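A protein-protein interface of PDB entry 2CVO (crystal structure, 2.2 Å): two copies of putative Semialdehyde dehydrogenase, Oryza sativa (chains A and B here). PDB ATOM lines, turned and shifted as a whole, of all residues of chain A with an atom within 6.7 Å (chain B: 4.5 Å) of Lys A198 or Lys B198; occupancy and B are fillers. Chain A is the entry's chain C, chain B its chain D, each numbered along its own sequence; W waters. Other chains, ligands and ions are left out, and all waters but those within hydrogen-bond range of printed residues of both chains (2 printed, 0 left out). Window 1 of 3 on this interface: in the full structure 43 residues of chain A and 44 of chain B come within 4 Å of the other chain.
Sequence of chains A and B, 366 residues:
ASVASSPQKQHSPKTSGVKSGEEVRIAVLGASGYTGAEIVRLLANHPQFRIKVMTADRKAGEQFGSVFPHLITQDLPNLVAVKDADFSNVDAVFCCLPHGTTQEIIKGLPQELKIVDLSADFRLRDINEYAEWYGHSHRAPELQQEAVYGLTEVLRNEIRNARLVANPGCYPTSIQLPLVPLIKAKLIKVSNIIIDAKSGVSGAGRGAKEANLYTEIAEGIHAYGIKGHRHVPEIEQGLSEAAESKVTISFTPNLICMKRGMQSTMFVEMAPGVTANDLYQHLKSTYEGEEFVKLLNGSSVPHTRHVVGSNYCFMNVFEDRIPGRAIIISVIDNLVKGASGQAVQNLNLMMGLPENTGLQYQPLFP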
ATOM      1  N   TYR A 171      23.850  32.074  14.574  1.00  0.00           N
ATOM      2  CA  TYR A 171      22.687  32.947  14.412  1.00  0.00           C
ATOM      3  C   TYR A 171      22.953  34.032  13.361  1.00  0.00           C
ATOM      4  O   TYR A 171      22.139  34.249  12.463  1.00  0.00           O
ATOM      5  CB  TYR A 171      22.317  33.623  15.739  1.00  0.00           C
ATOM      6  CG  TYR A 171      21.617  32.729  16.739  1.00  0.00           C
ATOM      7  CD1 TYR A 171      20.367  32.167  16.455  1.00  0.00           C
ATOM      8  CD2 TYR A 171      22.178  32.488  17.993  1.00  0.00           C
ATOM      9  CE1 TYR A 171      19.692  31.390  17.404  1.00  0.00           C
ATOM     10  CE2 TYR A 171      21.516  31.718  18.946  1.00  0.00           C
ATOM     11  CZ  TYR A 171      20.275  31.175  18.649  1.00  0.00           C
ATOM     12  OH  TYR A 171      19.612  30.445  19.609  1.00  0.00           O
ATOM     13  N   ASP A 196      13.026  36.305  15.984  1.00  0.00           N
ATOM     14  CA  ASP A 196      12.858  35.268  16.991  1.00  0.00           C
ATOM     15  C   ASP A 196      13.655  34.095  16.454  1.00  0.00           C
ATOM     16  O   ASP A 196      13.268  33.485  15.457  1.00  0.00           O
ATOM     17  CB  ASP A 196      11.402  34.849  17.149  1.00  0.00           C
ATOM     18  CG  ASP A 196      11.213  33.893  18.305  1.00  0.00           C
ATOM     19  OD1 ASP A 196      10.959  34.367  19.429  1.00  0.00           O
ATOM     20  OD2 ASP A 196      11.353  32.668  18.102  1.00  0.00           O
ATOM     21  N   ALA A 197      14.771  33.790  17.106  1.00  0.00           N
ATOM     22  CA  ALA A 197      15.636  32.703  16.654  1.00  0.00           C
ATOM     23  C   ALA A 197      15.590  31.478  17.560  1.00  0.00           C
ATOM     24  O   ALA A 197      15.479  31.594  18.784  1.00  0.00           O
ATOM     25  CB  ALA A 197      17.061  33.208  16.528  1.00  0.00           C
ATOM     26  N   LYS A 198      15.688  30.303  16.943  1.00  0.00           N
ATOM     27  CA  LYS A 198      15.636  29.036  17.662  1.00  0.00           C
ATOM     28  C   LYS A 198      16.861  28.191  17.333  1.00  0.00           C
ATOM     29  O   LYS A 198      17.288  28.126  16.178  1.00  0.00           O
ATOM     30  CB  LYS A 198      14.376  28.253  17.269  1.00  0.00           C
ATOM     31  CG  LYS A 198      13.041  28.983  17.478  1.00  0.00           C
ATOM     32  CD  LYS A 198      12.887  30.173  16.548  1.00  0.00           C
ATOM     33  CE  LYS A 198      11.527  30.190  15.859  1.00  0.00           C
ATOM     34  NZ  LYS A 198      10.396  30.202  16.819  1.00  0.00           N
ATOM     35  N   SER A 199      17.425  27.536  18.343  1.00  0.00           N
ATOM     36  CA  SER A 199      18.594  26.702  18.110  1.00  0.00           C
ATOM     37  C   SER A 199      18.648  25.449  18.962  1.00  0.00           C
ATOM     38  O   SER A 199      18.158  25.428  20.095  1.00  0.00           O
ATOM     39  CB  SER A 199      19.870  27.499  18.357  1.00  0.00           C
ATOM     40  OG  SER A 199      21.006  26.661  18.241  1.00  0.00           O
ATOM     41  N   GLY A 200      19.255  24.409  18.397  1.00  0.00           N
ATOM     42  CA  GLY A 200      19.430  23.163  19.115  1.00  0.00           C
ATOM     43  C   GLY A 200      20.448  23.440  20.203  1.00  0.00           C
ATOM     44  O   GLY A 200      21.248  24.373  20.086  1.00  0.00           O
ATOM     45  N   ILE A 221      11.053  24.099  25.963  1.00  0.00           N
ATOM     46  CA  ILE A 221      11.863  25.157  25.370  1.00  0.00           C
ATOM     47  C   ILE A 221      11.837  26.394  26.261  1.00  0.00           C
ATOM     48  O   ILE A 221      11.080  26.459  27.230  1.00  0.00           O
ATOM     49  CB  ILE A 221      11.314  25.566  23.986  1.00  0.00           C
ATOM     50  CG1 ILE A 221       9.892  26.115  24.146  1.00  0.00           C
ATOM     51  CG2 ILE A 221      11.310  24.365  23.044  1.00  0.00           C
ATOM     52  CD1 ILE A 221       9.330  26.762  22.902  1.00  0.00           C
ATOM     53  N   THR A 252      15.823  37.783  19.826  1.00  0.00           N
ATOM     54  CA  THR A 252      15.499  36.915  20.953  1.00  0.00           C
ATOM     55  C   THR A 252      15.739  35.452  20.596  1.00  0.00           C
ATOM     56  O   THR A 252      15.001  34.861  19.797  1.00  0.00           O
ATOM     57  CB  THR A 252      14.031  37.084  21.389  1.00  0.00           C
ATOM     58  OG1 THR A 252      13.780  38.460  21.692  1.00  0.00           O
ATOM     59  CG2 THR A 252      13.744  36.238  22.627  1.00  0.00           C
ATOM     60  N   PRO A 253      16.794  34.856  21.166  1.00  0.00           N
ATOM     61  CA  PRO A 253      17.123  33.455  20.902  1.00  0.00           C
ATOM     62  C   PRO A 253      16.327  32.529  21.819  1.00  0.00           C
ATOM     63  O   PRO A 253      15.914  32.930  22.907  1.00  0.00           O
ATOM     64  CB  PRO A 253      18.622  33.406  21.175  1.00  0.00           C
ATOM     65  CG  PRO A 253      18.758  34.352  22.331  1.00  0.00           C
ATOM     66  CD  PRO A 253      17.878  35.520  21.914  1.00  0.00           C
ATOM     67  N   ASN A 254      16.113  31.295  21.372  1.00  0.00           N
ATOM     68  CA  ASN A 254      15.358  30.307  22.140  1.00  0.00           C
ATOM     69  C   ASN A 254      16.066  28.950  22.080  1.00  0.00           C
ATOM     70  O   ASN A 254      16.437  28.484  21.003  1.00  0.00           O
ATOM     71  CB  ASN A 254      13.946  30.174  21.562  1.00  0.00           C
ATOM     72  CG  ASN A 254      13.169  31.484  21.589  1.00  0.00           C
ATOM     73  OD1 ASN A 254      12.465  31.785  22.555  1.00  0.00           O
ATOM     74  ND2 ASN A 254      13.300  32.271  20.528  1.00  0.00           N
ATOM     75  N   LEU A 255      16.249  28.320  23.236  1.00  0.00           N
ATOM     76  CA  LEU A 255      16.915  27.020  23.293  1.00  0.00           C
ATOM     77  C   LEU A 255      15.893  25.898  23.066  1.00  0.00           C
ATOM     78  O   LEU A 255      14.971  25.704  23.863  1.00  0.00           O
ATOM     79  CB  LEU A 255      17.612  26.856  24.646  1.00  0.00           C
ATOM     80  CG  LEU A 255      18.751  25.832  24.718  1.00  0.00           C
ATOM     81  CD1 LEU A 255      19.796  26.167  23.663  1.00  0.00           C
ATOM     82  CD2 LEU A 255      19.387  25.849  26.103  1.00  0.00           C
ATOM     83  N   ILE A 256      16.068  25.158  21.976  1.00  0.00           N
ATOM     84  CA  ILE A 256      15.152  24.081  21.621  1.00  0.00           C
ATOM     85  C   ILE A 256      15.626  22.692  22.034  1.00  0.00           C
ATOM     86  O   ILE A 256      16.830  22.409  22.049  1.00  0.00           O
ATOM     87  CB  ILE A 256      14.905  24.058  20.101  1.00  0.00           C
ATOM     88  CG1 ILE A 256      14.529  25.461  19.609  1.00  0.00           C
ATOM     89  CG2 ILE A 256      13.795  23.072  19.768  1.00  0.00           C
ATOM     90  CD1 ILE A 256      13.264  26.024  20.256  1.00  0.00           C
ATOM     91  N   MET A 258      16.498  19.859  20.963  1.00  0.00           N
ATOM     92  CA  MET A 258      17.031  19.112  19.831  1.00  0.00           C
ATOM     93  C   MET A 258      18.519  19.402  19.834  1.00  0.00           C
ATOM     94  O   MET A 258      18.942  20.453  20.311  1.00  0.00           O
ATOM     95  CB  MET A 258      16.402  19.574  18.511  1.00  0.00           C
ATOM     96  CG  MET A 258      16.653  21.033  18.139  1.00  0.00           C
ATOM     97  SD  MET A 258      15.601  21.513  16.739  1.00  0.00           S
ATOM     98  CE  MET A 258      16.427  23.045  16.163  1.00  0.00           C
ATOM     99  N   GLY A 261      20.411  21.980  14.458  1.00  0.00           N
ATOM    100  CA  GLY A 261      19.379  22.741  13.785  1.00  0.00           C
ATOM    101  C   GLY A 261      19.194  24.136  14.337  1.00  0.00           C
ATOM    102  O   GLY A 261      19.270  24.362  15.546  1.00  0.00           O
ATOM    103  N   MET A 262      18.947  25.077  13.435  1.00  0.00           N
ATOM    104  CA  MET A 262      18.742  26.460  13.823  1.00  0.00           C
ATOM    105  C   MET A 262      17.772  27.118  12.857  1.00  0.00           C
ATOM    106  O   MET A 262      17.821  26.886  11.647  1.00  0.00           O
ATOM    107  CB  MET A 262      20.079  27.211  13.824  1.00  0.00           C
ATOM    108  CG  MET A 262      19.953  28.717  14.022  1.00  0.00           C
ATOM    109  SD  MET A 262      21.577  29.512  14.197  1.00  0.00           S
ATOM    110  CE  MET A 262      21.927  29.180  15.956  1.00  0.00           C
ATOM    111  N   GLN A 263      16.874  27.925  13.403  1.00  0.00           N
ATOM    112  CA  GLN A 263      15.907  28.636  12.586  1.00  0.00           C
ATOM    113  C   GLN A 263      15.785  30.065  13.078  1.00  0.00           C
ATOM    114  O   GLN A 263      15.605  30.311  14.272  1.00  0.00           O
ATOM    115  CB  GLN A 263      14.526  27.972  12.641  1.00  0.00           C
ATOM    116  CG  GLN A 263      13.431  28.834  12.000  1.00  0.00           C
ATOM    117  CD  GLN A 263      12.052  28.188  12.015  1.00  0.00           C
ATOM    118  OE1 GLN A 263      11.035  28.882  12.046  1.00  0.00           O
ATOM    119  NE2 GLN A 263      12.010  26.864  11.970  1.00  0.00           N
ATOM    120  N   SER A 264      15.908  31.006  12.152  1.00  0.00           N
ATOM    121  CA  SER A 264      15.769  32.405  12.485  1.00  0.00           C
ATOM    122  C   SER A 264      14.578  32.913  11.698  1.00  0.00           C
ATOM    123  O   SER A 264      14.483  32.694  10.485  1.00  0.00           O
ATOM    124  CB  SER A 264      17.024  33.192  12.103  1.00  0.00           C
ATOM    125  OG  SER A 264      18.122  32.829  12.922  1.00  0.00           O
ATOM    126  N   THR A 265      13.654  33.553  12.399  1.00  0.00           N
ATOM    127  CA  THR A 265      12.479  34.112  11.757  1.00  0.00           C
ATOM    128  C   THR A 265      12.587  35.616  11.913  1.00  0.00           C
ATOM    129  O   THR A 265      12.645  36.137  13.025  1.00  0.00           O
ATOM    130  CB  THR A 265      11.186  33.625  12.411  1.00  0.00           C
ATOM    131  OG1 THR A 265      11.148  32.191  12.376  1.00  0.00           O
ATOM    132  CG2 THR A 265       9.979  34.184  11.662  1.00  0.00           C
ATOM    133  N   THR A 304      14.192  22.826  10.032  1.00  0.00           N
ATOM    134  CA  THR A 304      15.585  22.686  10.450  1.00  0.00           C
ATOM    135  C   THR A 304      16.029  21.230  10.245  1.00  0.00           C
ATOM    136  O   THR A 304      17.205  20.955  10.017  1.00  0.00           O
ATOM    137  CB  THR A 304      15.792  23.020  11.946  1.00  0.00           C
ATOM    138  OG1 THR A 304      15.051  22.090  12.748  1.00  0.00           O
ATOM    139  CG2 THR A 304      15.346  24.443  12.259  1.00  0.00           C
ATOM    140  N   TYR B 171      -3.411  28.462  21.702  1.00  0.00           N
ATOM    141  CA  TYR B 171      -2.654  29.680  21.408  1.00  0.00           C
ATOM    142  C   TYR B 171      -3.403  30.916  21.943  1.00  0.00           C
ATOM    143  O   TYR B 171      -2.828  31.736  22.666  1.00  0.00           O
ATOM    144  CB  TYR B 171      -2.421  29.828  19.897  1.00  0.00           C
ATOM    145  CG  TYR B 171      -1.405  28.866  19.303  1.00  0.00           C
ATOM    146  CD1 TYR B 171      -0.065  28.887  19.713  1.00  0.00           C
ATOM    147  CD2 TYR B 171      -1.770  27.969  18.301  1.00  0.00           C
ATOM    148  CE1 TYR B 171       0.884  28.037  19.133  1.00  0.00           C
ATOM    149  CE2 TYR B 171      -0.832  27.118  17.711  1.00  0.00           C
ATOM    150  CZ  TYR B 171       0.493  27.158  18.132  1.00  0.00           C
ATOM    151  OH  TYR B 171       1.423  26.333  17.538  1.00  0.00           O
ATOM    152  N   ASP B 196       5.123  35.190  17.765  1.00  0.00           N
ATOM    153  CA  ASP B 196       5.761  33.959  17.318  1.00  0.00           C
ATOM    154  C   ASP B 196       5.409  32.935  18.390  1.00  0.00           C
ATOM    155  O   ASP B 196       5.864  33.032  19.530  1.00  0.00           O
ATOM    156  CB  ASP B 196       7.276  34.127  17.207  1.00  0.00           C
ATOM    157  CG  ASP B 196       7.947  32.917  16.592  1.00  0.00           C
ATOM    158  OD1 ASP B 196       8.174  31.919  17.305  1.00  0.00           O
ATOM    159  OD2 ASP B 196       8.234  32.957  15.381  1.00  0.00           O
ATOM    160  N   ALA B 197       4.575  31.965  18.030  1.00  0.00           N
ATOM    161  CA  ALA B 197       4.139  30.957  18.988  1.00  0.00           C
ATOM    162  C   ALA B 197       4.702  29.584  18.672  1.00  0.00           C
ATOM    163  O   ALA B 197       4.926  29.236  17.507  1.00  0.00           O
ATOM    164  CB  ALA B 197       2.620  30.911  19.033  1.00  0.00           C
ATOM    165  N   LYS B 198       4.910  28.807  19.728  1.00  0.00           N
ATOM    166  CA  LYS B 198       5.488  27.477  19.620  1.00  0.00           C
ATOM    167  C   LYS B 198       4.644  26.475  20.407  1.00  0.00           C
ATOM    168  O   LYS B 198       4.195  26.758  21.516  1.00  0.00           O
ATOM    169  CB  LYS B 198       6.918  27.532  20.160  1.00  0.00           C
ATOM    170  CG  LYS B 198       7.692  28.748  19.632  1.00  0.00           C
ATOM    171  CD  LYS B 198       8.933  29.061  20.451  1.00  0.00           C
ATOM    172  CE  LYS B 198       9.680  30.271  19.891  1.00  0.00           C
ATOM    173  NZ  LYS B 198       8.835  31.507  19.856  1.00  0.00           N
ATOM    174  N   SER B 199       4.420  25.301  19.833  1.00  0.00           N
ATOM    175  CA  SER B 199       3.610  24.302  20.509  1.00  0.00           C
ATOM    176  C   SER B 199       4.103  22.879  20.324  1.00  0.00           C
ATOM    177  O   SER B 199       4.689  22.542  19.294  1.00  0.00           O
ATOM    178  CB  SER B 199       2.169  24.387  20.009  1.00  0.00           C
ATOM    179  OG  SER B 199       1.397  23.326  20.531  1.00  0.00           O
ATOM    180  N   ILE B 221      12.268  21.471  13.992  1.00  0.00           N
ATOM    181  CA  ILE B 221      11.105  22.347  14.137  1.00  0.00           C
ATOM    182  C   ILE B 221      10.776  23.018  12.803  1.00  0.00           C
ATOM    183  O   ILE B 221      11.585  23.018  11.876  1.00  0.00           O
ATOM    184  CB  ILE B 221      11.364  23.472  15.166  1.00  0.00           C
ATOM    185  CG1 ILE B 221      12.494  24.376  14.661  1.00  0.00           C
ATOM    186  CG2 ILE B 221      11.724  22.869  16.534  1.00  0.00           C
ATOM    187  CD1 ILE B 221      12.809  25.560  15.575  1.00  0.00           C
ATOM    188  N   ASN B 254       4.624  27.550  15.351  1.00  0.00           N
ATOM    189  CA  ASN B 254       5.753  26.688  15.010  1.00  0.00           C
ATOM    190  C   ASN B 254       5.546  25.347  15.712  1.00  0.00           C
ATOM    191  O   ASN B 254       5.227  25.312  16.895  1.00  0.00           O
ATOM    192  CB  ASN B 254       7.067  27.333  15.481  1.00  0.00           C
ATOM    193  CG  ASN B 254       7.355  28.673  14.791  1.00  0.00           C
ATOM    194  OD1 ASN B 254       8.023  28.724  13.764  1.00  0.00           O
ATOM    195  ND2 ASN B 254       6.838  29.758  15.358  1.00  0.00           N
ATOM    196  N   ILE B 256       6.893  22.285  17.498  1.00  0.00           N
ATOM    197  CA  ILE B 256       8.112  21.886  18.201  1.00  0.00           C
ATOM    198  C   ILE B 256       8.218  20.386  18.455  1.00  0.00           C
ATOM    199  O   ILE B 256       7.210  19.691  18.620  1.00  0.00           O
ATOM    200  CB  ILE B 256       8.223  22.616  19.566  1.00  0.00           C
ATOM    201  CG1 ILE B 256       8.087  24.128  19.369  1.00  0.00           C
ATOM    202  CG2 ILE B 256       9.559  22.300  20.224  1.00  0.00           C
ATOM    203  CD1 ILE B 256       9.156  24.735  18.468  1.00  0.00           C
ATOM    204  N   GLY B 261       3.378  21.387  25.951  1.00  0.00           N
ATOM    205  CA  GLY B 261       4.005  22.682  26.104  1.00  0.00           C
ATOM    206  C   GLY B 261       3.688  23.653  24.992  1.00  0.00           C
ATOM    207  O   GLY B 261       3.579  23.282  23.818  1.00  0.00           O
ATOM    208  N   MET B 262       3.547  24.912  25.375  1.00  0.00           N
ATOM    209  CA  MET B 262       3.251  25.967  24.426  1.00  0.00           C
ATOM    210  C   MET B 262       3.822  27.272  24.942  1.00  0.00           C
ATOM    211  O   MET B 262       3.700  27.594  26.128  1.00  0.00           O
ATOM    212  CB  MET B 262       1.741  26.102  24.246  1.00  0.00           C
ATOM    213  CG  MET B 262       1.307  27.336  23.467  1.00  0.00           C
ATOM    214  SD  MET B 262      -0.450  27.258  23.070  1.00  0.00           S
ATOM    215  CE  MET B 262      -0.446  26.092  21.678  1.00  0.00           C
ATOM    216  N   GLN B 263       4.454  28.018  24.045  1.00  0.00           N
ATOM    217  CA  GLN B 263       5.030  29.304  24.398  1.00  0.00           C
ATOM    218  C   GLN B 263       4.722  30.341  23.334  1.00  0.00           C
ATOM    219  O   GLN B 263       5.052  30.160  22.165  1.00  0.00           O
ATOM    220  CB  GLN B 263       6.551  29.206  24.556  1.00  0.00           C
ATOM    221  CG  GLN B 263       7.222  30.570  24.699  1.00  0.00           C
ATOM    222  CD  GLN B 263       8.734  30.494  24.776  1.00  0.00           C
ATOM    223  OE1 GLN B 263       9.432  31.384  24.292  1.00  0.00           O
ATOM    224  NE2 GLN B 263       9.247  29.445  25.393  1.00  0.00           N
ATOM    225  N   THR B 265       5.329  34.250  22.195  1.00  0.00           N
ATOM    226  CA  THR B 265       6.162  35.415  22.424  1.00  0.00           C
ATOM    227  C   THR B 265       5.494  36.548  21.675  1.00  0.00           C
ATOM    228  O   THR B 265       5.213  36.443  20.481  1.00  0.00           O
ATOM    229  CB  THR B 265       7.590  35.220  21.902  1.00  0.00           C
ATOM    230  OG1 THR B 265       8.169  34.070  22.534  1.00  0.00           O
ATOM    231  CG2 THR B 265       8.441  36.445  22.224  1.00  0.00           C
HETATM  232  O   HOH W   1       8.738  31.372  13.260  1.00  0.00           O
HETATM  233  O   HOH W   2      10.876  33.777  22.019  1.00  0.00           O
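The side-chain carboxylate of Asp B196 is in salt-bridge range of the side-chain amino group of Lys A198 (2.8 Å).
The side-chain hydroxyl (OG1) of Thr A304 is in hydrogen-bond range of the backbone NH (N) of Ile B221 (3.1 Å).
The side-chain amide oxygen (OE1) of Gln A263 sits close to the side-chain amide oxygen (OD1) of Asn B254 (3.5 Å).
OD2 of Asp A196 sits close to OD1 of Asp B196 (3.4 Å).
NZ of Lys B198 is in salt-bridge range of OD2 of Asp A196.
OE1 of Gln A263 lies within hydrogen-bond range of OG1 of Thr A265 (3.3 Å).
The side-chain amide oxygen of Gln B263 sits at hydrogen-bond distance from the side-chain hydroxyl of Thr B265.
N of Ser B199 is in hydrogen-bond range of O of Asn B254.
OD2 of Asp A196 sits at hydrogen-bond distance from ND2 of Asn A254 (3.1 Å).
The backbone carbonyl oxygen (O) of Thr A252 sits at hydrogen-bond distance from the side-chain amide nitrogen (ND2) of Asn A254, 3.2 Å away.
N of Lys A198 is in hydrogen-bond range of O of Gln A263, 2.7 Å away.
Among the printed residues, merely in contact across the chains: Lys A198 with Lys B198, Lys A198 with Ile B221, Lys A198 with Asn B254, Ile A221 with Lys B198, Ile A221 with Ile B256, Ile A221 with Gln B263, Asn A254 with Gln B263, Ile A256 with Ile B221 and Gln A263 with Ile B221.
Printed residues of chain B within 4 Å of Lys A198: Asp B196 (2.8 Å), Lys B198 (3.2 Å), Ile B221 (3.5 Å) and Asn B254 (3.9 Å).
Of chain A, only Asp A196 (3.3 Å), Lys A198 (3.2 Å) and Ile A221 (3.4 Å) come within 4 Å of Lys B198.
Of the printed residues of chain B, Asp A196 touches Asp B196 (3.4 Å) and Lys B198 (3.3 Å).
Of the printed residues of chain A, Asp B196 touches Asp A196 (3.4 Å) and Lys A198 (2.8 Å).
Of the printed residues of chain B, Asn A254 touches Gln B263.
Printed residues of chain B within 4 Å of Gln A263: Ile B221 (3.7 Å) and Asn B254 (3.5 Å).
Ala B197 touches none of the printed residues of chain A.
Gly B261 touches none of the printed residues of chain A.
The nearest printed residue of chain B that does not touch Lys A198 is Ala B197 (5.6 Å).
The nearest residue of chain A that does not touch Lys B198 is Asn A254 (4.1 Å).
Hydrophobic or aromatic side chains of chain A that line the printed part of chain B: Ile A221 and Ile A256.
Among the printed residues, 14 pairs touch across the chains.
Among the printed residues, Asp or Glu carboxylates within 4 Å of a Lys or Arg side-chain nitrogen of the other chain: Asp A196 with Lys B198 and Lys A198 with Asp B196.
Asp A196 touches Lys B198, and with the chains exchanged Lys A198 touches Asp B196.
Lys A198 touches its own counterpart, Lys B198.
Lys A198 touches Ile B221, and with the chains exchanged Ile A221 touches Lys B198.
Asn A254 touches Gln B263, and with the chains exchanged Gln A263 touches Asn B254.
Of the 14 pairs that touch across the chains among the printed residues, 12 have their exchanged pair printed and touching as well.
Water W2 lies within hydrogen-bond range of OD1 of Asn A254 (2.6 Å), OD1 of Asp A196 (2.7 Å) and OG1 of Thr B265 (2.8 Å).
Water W1 lies within hydrogen-bond range of OG1 of Thr A265, OD2 of Asp B196 and OD1 of Asn B254.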
